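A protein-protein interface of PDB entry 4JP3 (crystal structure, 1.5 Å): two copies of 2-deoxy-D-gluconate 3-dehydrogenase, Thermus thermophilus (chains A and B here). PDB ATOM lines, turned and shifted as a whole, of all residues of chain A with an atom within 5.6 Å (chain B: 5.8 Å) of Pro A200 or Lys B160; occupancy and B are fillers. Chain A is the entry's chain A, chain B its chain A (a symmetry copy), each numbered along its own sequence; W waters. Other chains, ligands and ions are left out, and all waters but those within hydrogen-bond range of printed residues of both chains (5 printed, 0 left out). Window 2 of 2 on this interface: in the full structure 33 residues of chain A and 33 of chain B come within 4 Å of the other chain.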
ATOM      1  N   THR A 196      20.160 -19.626  10.417  1.00  0.00           N
ATOM      2  CA  THR A 196      20.450 -18.497   9.548  1.00  0.00           C
ATOM      3  C   THR A 196      19.431 -18.319   8.425  1.00  0.00           C
ATOM      4  O   THR A 196      19.192 -17.200   7.967  1.00  0.00           O
ATOM      5  CB  THR A 196      21.871 -18.628   8.968  1.00  0.00           C
ATOM      6  OG1 THR A 196      22.800 -18.792  10.048  1.00  0.00           O
ATOM      7  CG2 THR A 196      22.251 -17.382   8.184  1.00  0.00           C
ATOM      8  N   ARG A 198      16.472 -18.423   8.724  1.00  0.00           N
ATOM      9  CA  ARG A 198      15.341 -17.725   9.330  1.00  0.00           C
ATOM     10  C   ARG A 198      15.670 -16.288   9.730  1.00  0.00           C
ATOM     11  O   ARG A 198      14.833 -15.596  10.310  1.00  0.00           O
ATOM     12  CB  ARG A 198      14.847 -18.497  10.554  1.00  0.00           C
ATOM     13  CG  ARG A 198      14.217 -19.839  10.217  1.00  0.00           C
ATOM     14  CD  ARG A 198      14.074 -20.699  11.456  1.00  0.00           C
ATOM     15  NE  ARG A 198      13.228 -20.075  12.469  1.00  0.00           N
ATOM     16  CZ  ARG A 198      13.053 -20.562  13.693  1.00  0.00           C
ATOM     17  NH1 ARG A 198      13.668 -21.680  14.057  1.00  0.00           N
ATOM     18  NH2 ARG A 198      12.261 -19.934  14.553  1.00  0.00           N
ATOM     19  N   ILE A 199      16.890 -15.849   9.437  1.00  0.00           N
ATOM     20  CA  ILE A 199      17.300 -14.482   9.753  1.00  0.00           C
ATOM     21  C   ILE A 199      17.179 -13.677   8.461  1.00  0.00           C
ATOM     22  O   ILE A 199      17.973 -13.853   7.538  1.00  0.00           O
ATOM     23  CB  ILE A 199      18.770 -14.407  10.228  1.00  0.00           C
ATOM     24  CG1 ILE A 199      18.984 -15.305  11.446  1.00  0.00           C
ATOM     25  CG2 ILE A 199      19.127 -12.960  10.578  1.00  0.00           C
ATOM     26  CD1 ILE A 199      20.440 -15.393  11.888  1.00  0.00           C
ATOM     27  N   PRO A 200      16.175 -12.793   8.374  1.00  0.00           N
ATOM     28  CA  PRO A 200      15.985 -11.979   7.168  1.00  0.00           C
ATOM     29  C   PRO A 200      17.244 -11.267   6.676  1.00  0.00           C
ATOM     30  O   PRO A 200      17.491 -11.202   5.470  1.00  0.00           O
ATOM     31  CB  PRO A 200      14.882 -11.013   7.585  1.00  0.00           C
ATOM     32  CG  PRO A 200      14.037 -11.871   8.476  1.00  0.00           C
ATOM     33  CD  PRO A 200      15.079 -12.565   9.334  1.00  0.00           C
ATOM     34  N   MET A 201      18.043 -10.739   7.598  1.00  0.00           N
ATOM     35  CA  MET A 201      19.264 -10.050   7.201  1.00  0.00           C
ATOM     36  C   MET A 201      20.327 -10.999   6.650  1.00  0.00           C
ATOM     37  O   MET A 201      21.329 -10.552   6.091  1.00  0.00           O
ATOM     38  CB  MET A 201      19.811  -9.220   8.366  1.00  0.00           C
ATOM     39  CG  MET A 201      19.046  -7.910   8.550  1.00  0.00           C
ATOM     40  SD  MET A 201      19.650  -6.857   9.886  1.00  0.00           S
ATOM     41  CE  MET A 201      21.370  -6.613   9.381  1.00  0.00           C
ATOM     42  N   GLY A 202      20.104 -12.302   6.813  1.00  0.00           N
ATOM     43  CA  GLY A 202      21.020 -13.300   6.278  1.00  0.00           C
ATOM     44  C   GLY A 202      22.392 -13.450   6.906  1.00  0.00           C
ATOM     45  O   GLY A 202      23.280 -14.076   6.316  1.00  0.00           O
ATOM     46  N   ASP A 233      17.608  -8.770  16.646  1.00  0.00           N
ATOM     47  CA  ASP A 233      17.885 -10.073  16.051  1.00  0.00           C
ATOM     48  C   ASP A 233      17.915 -10.193  14.531  1.00  0.00           C
ATOM     49  O   ASP A 233      17.762 -11.297  14.003  1.00  0.00           O
ATOM     50  CB  ASP A 233      16.854 -11.067  16.582  1.00  0.00           C
ATOM     51  CG  ASP A 233      15.448 -10.770  16.075  1.00  0.00           C
ATOM     52  OD1 ASP A 233      15.276  -9.778  15.331  1.00  0.00           O
ATOM     53  OD2 ASP A 233      14.514 -11.526  16.419  1.00  0.00           O
ATOM     54  N   GLY A 234      18.093  -9.082  13.827  1.00  0.00           N
ATOM     55  CA  GLY A 234      18.156  -9.145  12.376  1.00  0.00           C
ATOM     56  C   GLY A 234      16.883  -9.621  11.701  1.00  0.00           C
ATOM     57  O   GLY A 234      16.894  -9.960  10.513  1.00  0.00           O
ATOM     58  N   GLY A 235      15.789  -9.654  12.460  1.00  0.00           N
ATOM     59  CA  GLY A 235      14.508 -10.073  11.919  1.00  0.00           C
ATOM     60  C   GLY A 235      14.120 -11.515  12.190  1.00  0.00           C
ATOM     61  O   GLY A 235      13.056 -11.962  11.758  1.00  0.00           O
ATOM     62  N   PHE A 236      14.966 -12.240  12.914  1.00  0.00           N
ATOM     63  CA  PHE A 236      14.712 -13.647  13.219  1.00  0.00           C
ATOM     64  C   PHE A 236      13.317 -13.950  13.764  1.00  0.00           C
ATOM     65  O   PHE A 236      12.602 -14.801  13.228  1.00  0.00           O
ATOM     66  CB  PHE A 236      15.754 -14.162  14.215  1.00  0.00           C
ATOM     67  CG  PHE A 236      15.583 -15.613  14.571  1.00  0.00           C
ATOM     68  CD1 PHE A 236      16.085 -16.612  13.741  1.00  0.00           C
ATOM     69  CD2 PHE A 236      14.902 -15.986  15.729  1.00  0.00           C
ATOM     70  CE1 PHE A 236      15.911 -17.960  14.058  1.00  0.00           C
ATOM     71  CE2 PHE A 236      14.724 -17.333  16.052  1.00  0.00           C
ATOM     72  CZ  PHE A 236      15.230 -18.319  15.214  1.00  0.00           C
ATOM     73  N   ALA A 238      10.643 -12.138  13.710  1.00  0.00           N
ATOM     74  CA  ALA A 238       9.589 -11.682  12.813  1.00  0.00           C
ATOM     75  C   ALA A 238       9.352 -12.610  11.621  1.00  0.00           C
ATOM     76  O   ALA A 238       8.232 -12.710  11.124  1.00  0.00           O
ATOM     77  CB  ALA A 238       9.916 -10.281  12.311  1.00  0.00           C
ATOM     78  N   TYR A 239      10.411 -13.278  11.174  1.00  0.00           N
ATOM     79  CA  TYR A 239      10.371 -14.177  10.019  1.00  0.00           C
ATOM     80  C   TYR A 239       9.068 -14.956   9.849  1.00  0.00           C
ATOM     81  O   TYR A 239       8.718 -15.741  10.756  1.00  0.00           O
ATOM     82  CB  TYR A 239      11.553 -15.149  10.089  1.00  0.00           C
ATOM     83  CG  TYR A 239      11.720 -16.041   8.880  1.00  0.00           C
ATOM     84  CD1 TYR A 239      12.004 -15.505   7.623  1.00  0.00           C
ATOM     85  CD2 TYR A 239      11.622 -17.424   8.998  1.00  0.00           C
ATOM     86  CE1 TYR A 239      12.192 -16.329   6.515  1.00  0.00           C
ATOM     87  CE2 TYR A 239      11.806 -18.257   7.898  1.00  0.00           C
ATOM     88  CZ  TYR A 239      12.092 -17.704   6.663  1.00  0.00           C
ATOM     89  OH  TYR A 239      12.288 -18.529   5.581  1.00  0.00           O
ATOM     90  OXT TYR A 239       8.416 -14.773   8.797  1.00  0.00           O
ATOM     91  N   THR B 155       4.604  -4.681  10.057  1.00  0.00           N
ATOM     92  CA  THR B 155       5.993  -4.431  10.422  1.00  0.00           C
ATOM     93  C   THR B 155       6.830  -5.689  10.215  1.00  0.00           C
ATOM     94  O   THR B 155       7.896  -5.644   9.601  1.00  0.00           O
ATOM     95  CB  THR B 155       6.099  -3.980  11.897  1.00  0.00           C
ATOM     96  OG1 THR B 155       5.475  -2.696  12.047  1.00  0.00           O
ATOM     97  CG2 THR B 155       7.558  -3.883  12.333  1.00  0.00           C
ATOM     98  N   ARG B 156       6.345  -6.816  10.727  1.00  0.00           N
ATOM     99  CA  ARG B 156       7.061  -8.077  10.580  1.00  0.00           C
ATOM    100  C   ARG B 156       7.180  -8.477   9.114  1.00  0.00           C
ATOM    101  O   ARG B 156       8.248  -8.879   8.655  1.00  0.00           O
ATOM    102  CB  ARG B 156       6.340  -9.188  11.344  1.00  0.00           C
ATOM    103  CG  ARG B 156       6.367  -9.028  12.853  1.00  0.00           C
ATOM    104  CD  ARG B 156       5.380  -9.977  13.512  1.00  0.00           C
ATOM    105  NE  ARG B 156       5.406  -9.858  14.966  1.00  0.00           N
ATOM    106  CZ  ARG B 156       4.371 -10.116  15.755  1.00  0.00           C
ATOM    107  NH1 ARG B 156       3.213 -10.505  15.234  1.00  0.00           N
ATOM    108  NH2 ARG B 156       4.495  -9.989  17.067  1.00  0.00           N
ATOM    109  N   ALA B 157       6.075  -8.362   8.385  1.00  0.00           N
ATOM    110  CA  ALA B 157       6.039  -8.735   6.974  1.00  0.00           C
ATOM    111  C   ALA B 157       7.003  -7.936   6.107  1.00  0.00           C
ATOM    112  O   ALA B 157       7.747  -8.507   5.308  1.00  0.00           O
ATOM    113  CB  ALA B 157       4.618  -8.594   6.437  1.00  0.00           C
ATOM    114  N   LEU B 158       6.993  -6.617   6.257  1.00  0.00           N
ATOM    115  CA  LEU B 158       7.880  -5.783   5.457  1.00  0.00           C
ATOM    116  C   LEU B 158       9.332  -5.941   5.897  1.00  0.00           C
ATOM    117  O   LEU B 158      10.242  -5.937   5.069  1.00  0.00           O
ATOM    118  CB  LEU B 158       7.454  -4.314   5.539  1.00  0.00           C
ATOM    119  CG  LEU B 158       6.031  -4.007   5.054  1.00  0.00           C
ATOM    120  CD1 LEU B 158       5.807  -2.498   5.081  1.00  0.00           C
ATOM    121  CD2 LEU B 158       5.823  -4.553   3.641  1.00  0.00           C
ATOM    122  N   ALA B 159       9.553  -6.088   7.199  1.00  0.00           N
ATOM    123  CA  ALA B 159      10.911  -6.265   7.700  1.00  0.00           C
ATOM    124  C   ALA B 159      11.515  -7.520   7.080  1.00  0.00           C
ATOM    125  O   ALA B 159      12.668  -7.521   6.648  1.00  0.00           O
ATOM    126  CB  ALA B 159      10.896  -6.390   9.222  1.00  0.00           C
ATOM    127  N   LYS B 160      10.724  -8.587   7.030  1.00  0.00           N
ATOM    128  CA  LYS B 160      11.184  -9.852   6.475  1.00  0.00           C
ATOM    129  C   LYS B 160      11.580  -9.747   5.011  1.00  0.00           C
ATOM    130  O   LYS B 160      12.618 -10.262   4.599  1.00  0.00           O
ATOM    131  CB  LYS B 160      10.096 -10.924   6.613  1.00  0.00           C
ATOM    132  CG  LYS B 160      10.539 -12.295   6.118  1.00  0.00           C
ATOM    133  CD  LYS B 160       9.395 -13.298   6.024  1.00  0.00           C
ATOM    134  CE  LYS B 160       8.388 -12.913   4.955  1.00  0.00           C
ATOM    135  NZ  LYS B 160       7.449 -14.034   4.648  1.00  0.00           N
ATOM    136  N   GLU B 161      10.757  -9.067   4.225  1.00  0.00           N
ATOM    137  CA  GLU B 161      11.026  -8.952   2.799  1.00  0.00           C
ATOM    138  C   GLU B 161      12.087  -7.946   2.394  1.00  0.00           C
ATOM    139  O   GLU B 161      12.745  -8.123   1.368  1.00  0.00           O
ATOM    140  CB  GLU B 161       9.735  -8.622   2.049  1.00  0.00           C
ATOM    141  CG  GLU B 161       8.608  -9.590   2.331  1.00  0.00           C
ATOM    142  CD  GLU B 161       7.448  -9.435   1.374  1.00  0.00           C
ATOM    143  OE1 GLU B 161       7.275  -8.331   0.805  1.00  0.00           O
ATOM    144  OE2 GLU B 161       6.702 -10.424   1.208  1.00  0.00           O
ATOM    145  N   TRP B 162      12.271  -6.902   3.191  1.00  0.00           N
ATOM    146  CA  TRP B 162      13.224  -5.862   2.826  1.00  0.00           C
ATOM    147  C   TRP B 162      14.554  -5.835   3.571  1.00  0.00           C
ATOM    148  O   TRP B 162      15.392  -4.973   3.308  1.00  0.00           O
ATOM    149  CB  TRP B 162      12.541  -4.493   2.934  1.00  0.00           C
ATOM    150  CG  TRP B 162      11.283  -4.372   2.104  1.00  0.00           C
ATOM    151  CD1 TRP B 162      10.915  -5.158   1.047  1.00  0.00           C
ATOM    152  CD2 TRP B 162      10.249  -3.388   2.246  1.00  0.00           C
ATOM    153  NE1 TRP B 162       9.719  -4.727   0.525  1.00  0.00           N
ATOM    154  CE2 TRP B 162       9.287  -3.642   1.241  1.00  0.00           C
ATOM    155  CE3 TRP B 162      10.042  -2.316   3.124  1.00  0.00           C
ATOM    156  CZ2 TRP B 162       8.135  -2.861   1.089  1.00  0.00           C
ATOM    157  CZ3 TRP B 162       8.894  -1.538   2.972  1.00  0.00           C
ATOM    158  CH2 TRP B 162       7.957  -1.818   1.961  1.00  0.00           C
ATOM    159  N   ALA B 163      14.757  -6.780   4.483  1.00  0.00           N
ATOM    160  CA  ALA B 163      15.996  -6.839   5.254  1.00  0.00           C
ATOM    161  C   ALA B 163      17.239  -6.888   4.366  1.00  0.00           C
ATOM    162  O   ALA B 163      18.209  -6.170   4.607  1.00  0.00           O
ATOM    163  CB  ALA B 163      15.973  -8.050   6.181  1.00  0.00           C
ATOM    164  N   ARG B 164      17.207  -7.737   3.341  1.00  0.00           N
ATOM    165  CA  ARG B 164      18.338  -7.885   2.430  1.00  0.00           C
ATOM    166  C   ARG B 164      18.616  -6.628   1.611  1.00  0.00           C
ATOM    167  O   ARG B 164      19.706  -6.473   1.056  1.00  0.00           O
ATOM    168  CB  ARG B 164      18.092  -9.056   1.479  1.00  0.00           C
ATOM    169  CG  ARG B 164      18.048 -10.418   2.146  1.00  0.00           C
ATOM    170  CD  ARG B 164      19.441 -10.969   2.381  1.00  0.00           C
ATOM    171  NE  ARG B 164      19.400 -12.376   2.766  1.00  0.00           N
ATOM    172  CZ  ARG B 164      20.455 -13.180   2.774  1.00  0.00           C
ATOM    173  NH1 ARG B 164      21.646 -12.720   2.416  1.00  0.00           N
ATOM    174  NH2 ARG B 164      20.321 -14.450   3.138  1.00  0.00           N
ATOM    175  N   THR B 226      15.186  -5.114  13.518  1.00  0.00           N
ATOM    176  CA  THR B 226      14.122  -5.005  12.533  1.00  0.00           C
ATOM    177  C   THR B 226      12.991  -6.010  12.754  1.00  0.00           C
ATOM    178  O   THR B 226      13.212  -7.107  13.275  1.00  0.00           O
ATOM    179  CB  THR B 226      14.697  -5.157  11.099  1.00  0.00           C
ATOM    180  OG1 THR B 226      13.698  -4.790  10.141  1.00  0.00           O
ATOM    181  CG2 THR B 226      15.152  -6.591  10.839  1.00  0.00           C
HETATM  182  O   HOH W   1      17.840 -13.767   4.325  1.00  0.00           O
HETATM  183  O   HOH W   2      12.593  -9.612  14.536  1.00  0.00           O
HETATM  184  O   HOH W   3      15.393  -7.045  15.792  1.00  0.00           O
HETATM  185  O   HOH W   4      22.595 -16.078   4.340  1.00  0.00           O
HETATM  186  O   HOH W   5      18.593 -15.923   5.555  1.00  0.00           O
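The side-chain carboxylate (OD1) of Asp A233 is in hydrogen-bond range of the backbone NH (N) of Phe A236, 3.5 Å away. The backbone NH (N) of Gly A235 is in hydrogen-bond range of the side-chain carboxylate (OD1) of Asp A233, at 2.9 Å. The backbone NH (N) of Met A201 lies within hydrogen-bond range of the backbone carbonyl oxygen (O) of Gly A234 (3.2 Å).
Pro A200 touches Lys B160 (CB to O, 3.8 Å). Ala B163 touches Pro A200. O of Pro A200 touches CG of Arg B164, at 3.5 Å. Ala B163 touches Met A201. CA of Gly A202 touches NH2 of Arg B164, 3.4 Å away. OD1 of Asp A233 touches O of Thr B226 (3.95 Å). Gly A234 touches Thr B226 (C to CG2, 3.6 Å). Thr B226 touches Gly A235 (O to CA, 3.5 Å). Arg B156 touches Ala A238. Tyr A239 touches Lys B160 (OXT to CD, 3.3 Å).
Printed residues of chain B within 4 Å of Pro A200: Lys B160, Ala B163 and Arg B164. Of the printed residues of chain B, Met A201 touches Ala B163 (3.7 Å). Printed residues of chain B within 4 Å of Asp A233: Thr B226. Of the printed residues of chain B, Gly A235 touches Thr B226. Phe A236 touches none of the printed residues of chain B. Printed residues of chain B within 4 Å of Tyr A239: Lys B160 (3.3 Å). Thr B155 touches none of the printed residues of chain A. Lys B160 touches just these residues of chain A: Pro A200 and Tyr A239. The nearest residue of chain A that does not touch Lys B160 is Ala A238 (5.2 Å).
Of the 11 printed residues of chain B, 5 touch a printed residue of chain A. Printed residues of chain B that touch a printed residue of chain A: Arg B156, Lys B160, Ala B163, Arg B164 and Thr B226. Hydrophobic or aromatic side chains of chain B within 4 Å of the printed part of chain A: Ala B163. Printed residues of chain A that touch a printed residue of chain B: Pro A200, Met A201, Gly A202, Asp A233, Gly A234, Gly A235, Ala A238 and Tyr A239. Along chain A the printed residues that touch a printed residue of chain B span positions 200 to 239. Among the printed residues, no Asp or Glu carboxylate lies within 4 Å of a Lys or Arg side-chain nitrogen of the other chain.
No position is printed for both chains. Of the 10 pairs that touch across the chains among the printed residues, none has its exchanged pair printed and touching as well.
Water W1 lies within hydrogen-bond range of the guanidinium group (NE) of Arg B164 (2.6 Å), the backbone carbonyl oxygen (O) of Pro A200 (2.8 Å) and the backbone carbonyl oxygen (O) of Ile A199 (3.2 Å). Water W3 bridges OD1 of Asp A233 (2.8 Å) and N of Thr B226 (3.0 Å). Water W5 lies within hydrogen-bond range of the backbone carbonyl oxygen (O) of Thr A196, the backbone carbonyl oxygen (O) of Ile A199 and the guanidinium group (NH2) of Arg B164. Water W2 lies within hydrogen-bond range of OD1 of Asp A233 (2.8 Å), O of Thr B226 (2.9 Å) and N of Ala A238 (3.3 Å). Water W4 lies within hydrogen-bond range of the backbone carbonyl oxygen of Gly A202 and the guanidinium group of Arg B164.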
